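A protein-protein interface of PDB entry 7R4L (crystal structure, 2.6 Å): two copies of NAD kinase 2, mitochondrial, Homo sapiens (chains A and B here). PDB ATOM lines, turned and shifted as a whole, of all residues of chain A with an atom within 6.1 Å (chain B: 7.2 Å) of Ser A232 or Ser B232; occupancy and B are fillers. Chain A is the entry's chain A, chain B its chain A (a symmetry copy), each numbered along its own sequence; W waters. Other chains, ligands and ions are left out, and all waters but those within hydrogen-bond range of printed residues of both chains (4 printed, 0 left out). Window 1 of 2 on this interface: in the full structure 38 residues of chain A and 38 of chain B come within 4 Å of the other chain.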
ATOM      1  N   GLY A 230      24.184  12.537 -13.052  1.00  0.00           N
ATOM      2  CA  GLY A 230      25.628  12.687 -13.006  1.00  0.00           C
ATOM      3  C   GLY A 230      26.051  13.707 -11.975  1.00  0.00           C
ATOM      4  O   GLY A 230      25.235  14.472 -11.444  1.00  0.00           O
ATOM      5  N   GLU A 231      27.357  13.689 -11.699  1.00  0.00           N
ATOM      6  CA  GLU A 231      27.982  14.677 -10.836  1.00  0.00           C
ATOM      7  C   GLU A 231      27.774  16.072 -11.399  1.00  0.00           C
ATOM      8  O   GLU A 231      27.777  16.287 -12.610  1.00  0.00           O
ATOM      9  CB  GLU A 231      29.493  14.406 -10.715  1.00  0.00           C
ATOM     10  CG  GLU A 231      29.856  13.164  -9.932  1.00  0.00           C
ATOM     11  CD  GLU A 231      29.748  13.358  -8.409  1.00  0.00           C
ATOM     12  OE1 GLU A 231      29.324  14.450  -7.955  1.00  0.00           O
ATOM     13  OE2 GLU A 231      30.101  12.418  -7.657  1.00  0.00           O
ATOM     14  N   SER A 232      27.599  17.026 -10.503  1.00  0.00           N
ATOM     15  CA  SER A 232      27.368  18.392 -10.926  1.00  0.00           C
ATOM     16  C   SER A 232      28.606  18.986 -11.569  1.00  0.00           C
ATOM     17  O   SER A 232      28.493  19.783 -12.503  1.00  0.00           O
ATOM     18  CB  SER A 232      26.957  19.212  -9.719  1.00  0.00           C
ATOM     19  OG  SER A 232      25.752  18.691  -9.211  1.00  0.00           O
ATOM     20  N   LEU A 233      29.789  18.623 -11.076  1.00  0.00           N
ATOM     21  CA  LEU A 233      31.036  19.166 -11.609  1.00  0.00           C
ATOM     22  C   LEU A 233      31.343  18.498 -12.943  1.00  0.00           C
ATOM     23  O   LEU A 233      31.478  17.268 -13.013  1.00  0.00           O
ATOM     24  CB  LEU A 233      32.169  18.940 -10.617  1.00  0.00           C
ATOM     25  CG  LEU A 233      33.440  19.733 -10.906  1.00  0.00           C
ATOM     26  CD1 LEU A 233      33.175  21.212 -10.765  1.00  0.00           C
ATOM     27  CD2 LEU A 233      34.573  19.309  -9.969  1.00  0.00           C
ATOM     28  N   SER A 234      31.444  19.302 -14.006  1.00  0.00           N
ATOM     29  CA  SER A 234      31.456  18.721 -15.348  1.00  0.00           C
ATOM     30  C   SER A 234      32.618  17.751 -15.558  1.00  0.00           C
ATOM     31  O   SER A 234      32.496  16.806 -16.343  1.00  0.00           O
ATOM     32  CB  SER A 234      31.393  19.811 -16.433  1.00  0.00           C
ATOM     33  OG  SER A 234      32.414  20.774 -16.277  1.00  0.00           O
ATOM     34  N   SER A 235      33.723  17.932 -14.837  1.00  0.00           N
ATOM     35  CA  SER A 235      34.939  17.168 -15.042  1.00  0.00           C
ATOM     36  C   SER A 235      35.120  16.045 -14.040  1.00  0.00           C
ATOM     37  O   SER A 235      36.162  15.395 -14.042  1.00  0.00           O
ATOM     38  CB  SER A 235      36.154  18.109 -15.002  1.00  0.00           C
ATOM     39  OG  SER A 235      36.364  18.616 -13.693  1.00  0.00           O
ATOM     40  N   ASP A 355      28.335  14.712  -5.130  1.00  0.00           N
ATOM     41  CA  ASP A 355      27.546  15.931  -5.315  1.00  0.00           C
ATOM     42  C   ASP A 355      26.886  15.853  -6.697  1.00  0.00           C
ATOM     43  O   ASP A 355      27.188  16.603  -7.637  1.00  0.00           O
ATOM     44  CB  ASP A 355      28.428  17.170  -5.167  1.00  0.00           C
ATOM     45  CG  ASP A 355      27.643  18.456  -5.229  1.00  0.00           C
ATOM     46  OD1 ASP A 355      26.441  18.449  -4.894  1.00  0.00           O
ATOM     47  OD2 ASP A 355      28.233  19.474  -5.638  1.00  0.00           O
ATOM     48  N   ALA A 356      25.953  14.915  -6.833  1.00  0.00           N
ATOM     49  CA  ALA A 356      25.359  14.590  -8.115  1.00  0.00           C
ATOM     50  C   ALA A 356      23.873  14.927  -8.136  1.00  0.00           C
ATOM     51  O   ALA A 356      23.236  15.095  -7.097  1.00  0.00           O
ATOM     52  CB  ALA A 356      25.556  13.107  -8.425  1.00  0.00           C
ATOM     53  N   CYS A 357      23.320  15.011  -9.344  1.00  0.00           N
ATOM     54  CA  CYS A 357      21.926  15.365  -9.541  1.00  0.00           C
ATOM     55  C   CYS A 357      21.266  14.444 -10.562  1.00  0.00           C
ATOM     56  O   CYS A 357      21.910  13.885 -11.456  1.00  0.00           O
ATOM     57  CB  CYS A 357      21.774  16.805 -10.048  1.00  0.00           C
ATOM     58  SG  CYS A 357      22.200  18.100  -8.869  1.00  0.00           S
ATOM     59  N   PHE B 228      39.236  21.157 -20.774  1.00  0.00           N
ATOM     60  CA  PHE B 228      37.813  21.045 -21.037  1.00  0.00           C
ATOM     61  C   PHE B 228      37.181  22.428 -20.935  1.00  0.00           C
ATOM     62  O   PHE B 228      37.569  23.242 -20.089  1.00  0.00           O
ATOM     63  CB  PHE B 228      37.136  20.103 -20.047  1.00  0.00           C
ATOM     64  CG  PHE B 228      35.651  20.065 -20.207  1.00  0.00           C
ATOM     65  CD1 PHE B 228      35.079  19.346 -21.255  1.00  0.00           C
ATOM     66  CD2 PHE B 228      34.822  20.792 -19.347  1.00  0.00           C
ATOM     67  CE1 PHE B 228      33.698  19.329 -21.430  1.00  0.00           C
ATOM     68  CE2 PHE B 228      33.442  20.779 -19.513  1.00  0.00           C
ATOM     69  CZ  PHE B 228      32.878  20.045 -20.557  1.00  0.00           C
ATOM     70  N   GLY B 230      33.279  24.271 -20.943  1.00  0.00           N
ATOM     71  CA  GLY B 230      31.838  24.099 -21.018  1.00  0.00           C
ATOM     72  C   GLY B 230      31.135  24.768 -19.861  1.00  0.00           C
ATOM     73  O   GLY B 230      31.757  25.177 -18.871  1.00  0.00           O
ATOM     74  N   GLU B 231      29.814  24.877 -20.019  1.00  0.00           N
ATOM     75  CA  GLU B 231      28.944  25.369 -18.964  1.00  0.00           C
ATOM     76  C   GLU B 231      29.066  24.490 -17.731  1.00  0.00           C
ATOM     77  O   GLU B 231      29.229  23.275 -17.817  1.00  0.00           O
ATOM     78  CB  GLU B 231      27.478  25.370 -19.434  1.00  0.00           C
ATOM     79  CG  GLU B 231      27.150  26.399 -20.493  1.00  0.00           C
ATOM     80  CD  GLU B 231      26.990  27.820 -19.922  1.00  0.00           C
ATOM     81  OE1 GLU B 231      27.199  28.022 -18.700  1.00  0.00           O
ATOM     82  OE2 GLU B 231      26.639  28.743 -20.697  1.00  0.00           O
ATOM     83  N   SER B 232      28.978  25.121 -16.574  1.00  0.00           N
ATOM     84  CA  SER B 232      29.104  24.388 -15.331  1.00  0.00           C
ATOM     85  C   SER B 232      27.921  23.466 -15.113  1.00  0.00           C
ATOM     86  O   SER B 232      28.082  22.376 -14.557  1.00  0.00           O
ATOM     87  CB  SER B 232      29.215  25.380 -14.189  1.00  0.00           C
ATOM     88  OG  SER B 232      30.378  26.150 -14.375  1.00  0.00           O
ATOM     89  N   LEU B 233      26.728  23.887 -15.530  1.00  0.00           N
ATOM     90  CA  LEU B 233      25.524  23.082 -15.336  1.00  0.00           C
ATOM     91  C   LEU B 233      25.518  21.942 -16.345  1.00  0.00           C
ATOM     92  O   LEU B 233      25.547  22.179 -17.562  1.00  0.00           O
ATOM     93  CB  LEU B 233      24.285  23.952 -15.494  1.00  0.00           C
ATOM     94  CG  LEU B 233      22.988  23.313 -15.005  1.00  0.00           C
ATOM     95  CD1 LEU B 233      23.044  23.094 -13.514  1.00  0.00           C
ATOM     96  CD2 LEU B 233      21.781  24.182 -15.366  1.00  0.00           C
ATOM     97  N   SER B 234      25.489  20.701 -15.848  1.00  0.00           N
ATOM     98  CA  SER B 234      25.761  19.566 -16.729  1.00  0.00           C
ATOM     99  C   SER B 234      24.774  19.477 -17.894  1.00  0.00           C
ATOM    100  O   SER B 234      25.135  18.986 -18.968  1.00  0.00           O
ATOM    101  CB  SER B 234      25.862  18.251 -15.937  1.00  0.00           C
ATOM    102  OG  SER B 234      24.718  18.024 -15.139  1.00  0.00           O
ATOM    103  N   SER B 235      23.556  19.984 -17.722  1.00  0.00           N
ATOM    104  CA  SER B 235      22.490  19.838 -18.696  1.00  0.00           C
ATOM    105  C   SER B 235      22.291  21.069 -19.559  1.00  0.00           C
ATOM    106  O   SER B 235      21.351  21.109 -20.347  1.00  0.00           O
ATOM    107  CB  SER B 235      21.179  19.482 -17.978  1.00  0.00           C
ATOM    108  OG  SER B 235      20.703  20.577 -17.210  1.00  0.00           O
ATOM    109  N   ARG B 236      23.116  22.087 -19.408  1.00  0.00           N
ATOM    110  CA  ARG B 236      22.986  23.311 -20.187  1.00  0.00           C
ATOM    111  C   ARG B 236      23.919  23.252 -21.388  1.00  0.00           C
ATOM    112  O   ARG B 236      25.135  23.083 -21.229  1.00  0.00           O
ATOM    113  CB  ARG B 236      23.296  24.553 -19.352  1.00  0.00           C
ATOM    114  CG  ARG B 236      22.970  25.802 -20.120  1.00  0.00           C
ATOM    115  CD  ARG B 236      23.648  27.036 -19.593  1.00  0.00           C
ATOM    116  NE  ARG B 236      23.286  27.224 -18.198  1.00  0.00           N
ATOM    117  CZ  ARG B 236      22.266  27.957 -17.769  1.00  0.00           C
ATOM    118  NH1 ARG B 236      21.445  28.571 -18.617  1.00  0.00           N
ATOM    119  NH2 ARG B 236      22.049  28.057 -16.457  1.00  0.00           N
ATOM    120  N   SER B 238      26.343  24.330 -24.251  1.00  0.00           N
ATOM    121  CA  SER B 238      27.383  25.341 -24.325  1.00  0.00           C
ATOM    122  C   SER B 238      27.429  25.953 -25.719  1.00  0.00           C
ATOM    123  O   SER B 238      27.253  25.258 -26.722  1.00  0.00           O
ATOM    124  CB  SER B 238      28.745  24.729 -23.983  1.00  0.00           C
ATOM    125  OG  SER B 238      28.751  24.160 -22.685  1.00  0.00           O
ATOM    126  N   CYS B 353      29.104  31.899 -23.356  1.00  0.00           N
ATOM    127  CA  CYS B 353      28.431  31.168 -22.295  1.00  0.00           C
ATOM    128  C   CYS B 353      27.981  32.094 -21.176  1.00  0.00           C
ATOM    129  O   CYS B 353      28.416  33.241 -21.054  1.00  0.00           O
ATOM    130  CB  CYS B 353      29.346  30.088 -21.720  1.00  0.00           C
ATOM    131  SG  CYS B 353      29.782  28.706 -22.801  1.00  0.00           S
ATOM    132  N   ASP B 355      27.687  30.780 -17.612  1.00  0.00           N
ATOM    133  CA  ASP B 355      28.340  30.381 -16.365  1.00  0.00           C
ATOM    134  C   ASP B 355      29.216  29.159 -16.667  1.00  0.00           C
ATOM    135  O   ASP B 355      28.977  28.026 -16.223  1.00  0.00           O
ATOM    136  CB  ASP B 355      27.301  30.091 -15.283  1.00  0.00           C
ATOM    137  CG  ASP B 355      27.923  29.793 -13.941  1.00  0.00           C
ATOM    138  OD1 ASP B 355      29.048  30.262 -13.677  1.00  0.00           O
ATOM    139  OD2 ASP B 355      27.285  29.063 -13.159  1.00  0.00           O
ATOM    140  N   ALA B 356      30.266  29.388 -17.450  1.00  0.00           N
ATOM    141  CA  ALA B 356      31.092  28.318 -17.976  1.00  0.00           C
ATOM    142  C   ALA B 356      32.510  28.392 -17.421  1.00  0.00           C
ATOM    143  O   ALA B 356      32.948  29.421 -16.910  1.00  0.00           O
ATOM    144  CB  ALA B 356      31.130  28.385 -19.501  1.00  0.00           C
ATOM    145  N   CYS B 357      33.233  27.281 -17.545  1.00  0.00           N
ATOM    146  CA  CYS B 357      34.587  27.170 -17.031  1.00  0.00           C
ATOM    147  C   CYS B 357      35.508  26.515 -18.054  1.00  0.00           C
ATOM    148  O   CYS B 357      35.087  25.726 -18.908  1.00  0.00           O
ATOM    149  CB  CYS B 357      34.640  26.329 -15.751  1.00  0.00           C
ATOM    150  SG  CYS B 357      33.876  27.067 -14.295  1.00  0.00           S
ATOM    151  N   SER B 365      40.411  25.328 -12.484  1.00  0.00           N
ATOM    152  CA  SER B 365      39.288  25.852 -13.231  1.00  0.00           C
ATOM    153  C   SER B 365      39.404  27.368 -13.371  1.00  0.00           C
ATOM    154  O   SER B 365      39.798  28.063 -12.432  1.00  0.00           O
ATOM    155  CB  SER B 365      37.982  25.470 -12.510  1.00  0.00           C
ATOM    156  OG  SER B 365      36.871  25.974 -13.214  1.00  0.00           O
ATOM    157  N   ASN B 369      33.286  33.159 -19.525  1.00  0.00           N
ATOM    158  CA  ASN B 369      31.937  33.556 -19.905  1.00  0.00           C
ATOM    159  C   ASN B 369      31.958  34.511 -21.090  1.00  0.00           C
ATOM    160  O   ASN B 369      33.013  34.941 -21.561  1.00  0.00           O
ATOM    161  CB  ASN B 369      31.170  34.144 -18.718  1.00  0.00           C
ATOM    162  CG  ASN B 369      30.970  33.134 -17.611  1.00  0.00           C
ATOM    163  OD1 ASN B 369      30.693  31.964 -17.872  1.00  0.00           O
ATOM    164  ND2 ASN B 369      31.122  33.573 -16.371  1.00  0.00           N
HETATM  165  O   HOH W   1      25.792  20.736 -12.908  1.00  0.00           O
HETATM  166  O   HOH W   2      24.095  16.735 -12.906  1.00  0.00           O
HETATM  167  O   HOH W   3      30.675  22.071 -13.313  1.00  0.00           O
HETATM  168  O   HOH W   4      32.828  23.325 -16.875  1.00  0.00           O
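O of Ser B232 sits close to O of Ser A232 (3.3 Å).
The backbone carbonyl oxygen (O) of Asp A355 is in hydrogen-bond range of the backbone NH (N) of Ser A232, at 2.9 Å. The side-chain hydroxyl of Ser A232 sits at hydrogen-bond distance from the side-chain sulfur of Cys A357, at 3.6 Å. N of Ser B232 lies within hydrogen-bond range of O of Asp B355. The side-chain hydroxyl of Ser B232 is in hydrogen-bond range of the side-chain sulfur of Cys B357.
Among the printed residues, merely in contact across the chains: Ser A234 with Phe B228.
Ser A232 touches just one residue of chain B: Ser B232. Of the printed residues of chain B, Ser A234 touches Phe B228 (3.4 Å). Printed residues of chain A within 4 Å of Phe B228: Ser A234 (3.4 Å). Ser B234 touches none of the printed residues of chain A. Ser B235 touches none of the printed residues of chain A. The nearest residue of chain B that does not touch Ser A232 is Ser B234 (4.6 Å).
Of the 9 printed residues of chain A, 2 touch a printed residue of chain B. Among the printed residues, 2 pairs touch across the chains. Among the printed residues, no Asp or Glu carboxylate lies within 4 Å of a Lys or Arg side-chain nitrogen of the other chain.
Ser A232 touches its own counterpart, Ser B232. 9 positions are printed for both chains. Of the 2 pairs that touch across the chains among the printed residues, 1 has its exchanged pair printed and touching as well.
Water W4 bridges the side-chain hydroxyl (OG) of Ser A234 and the backbone carbonyl oxygen (O) of Gly B230. Water W2 bridges the side-chain hydroxyl (OG) of Ser B234 (2.7 Å) and the backbone carbonyl oxygen (O) of Gly A230 (2.9 Å). Water W1 lies within hydrogen-bond range of the backbone carbonyl oxygen of Ser A232, the backbone NH of Ser B234 and the backbone carbonyl oxygen of Ser B232. Water W3 lies within hydrogen-bond range of the backbone carbonyl oxygen (O) of Ser B232 (2.9 Å), the backbone NH (N) of Ser A234 (3.0 Å) and the backbone carbonyl oxygen (O) of Ser A232 (3.3 Å).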
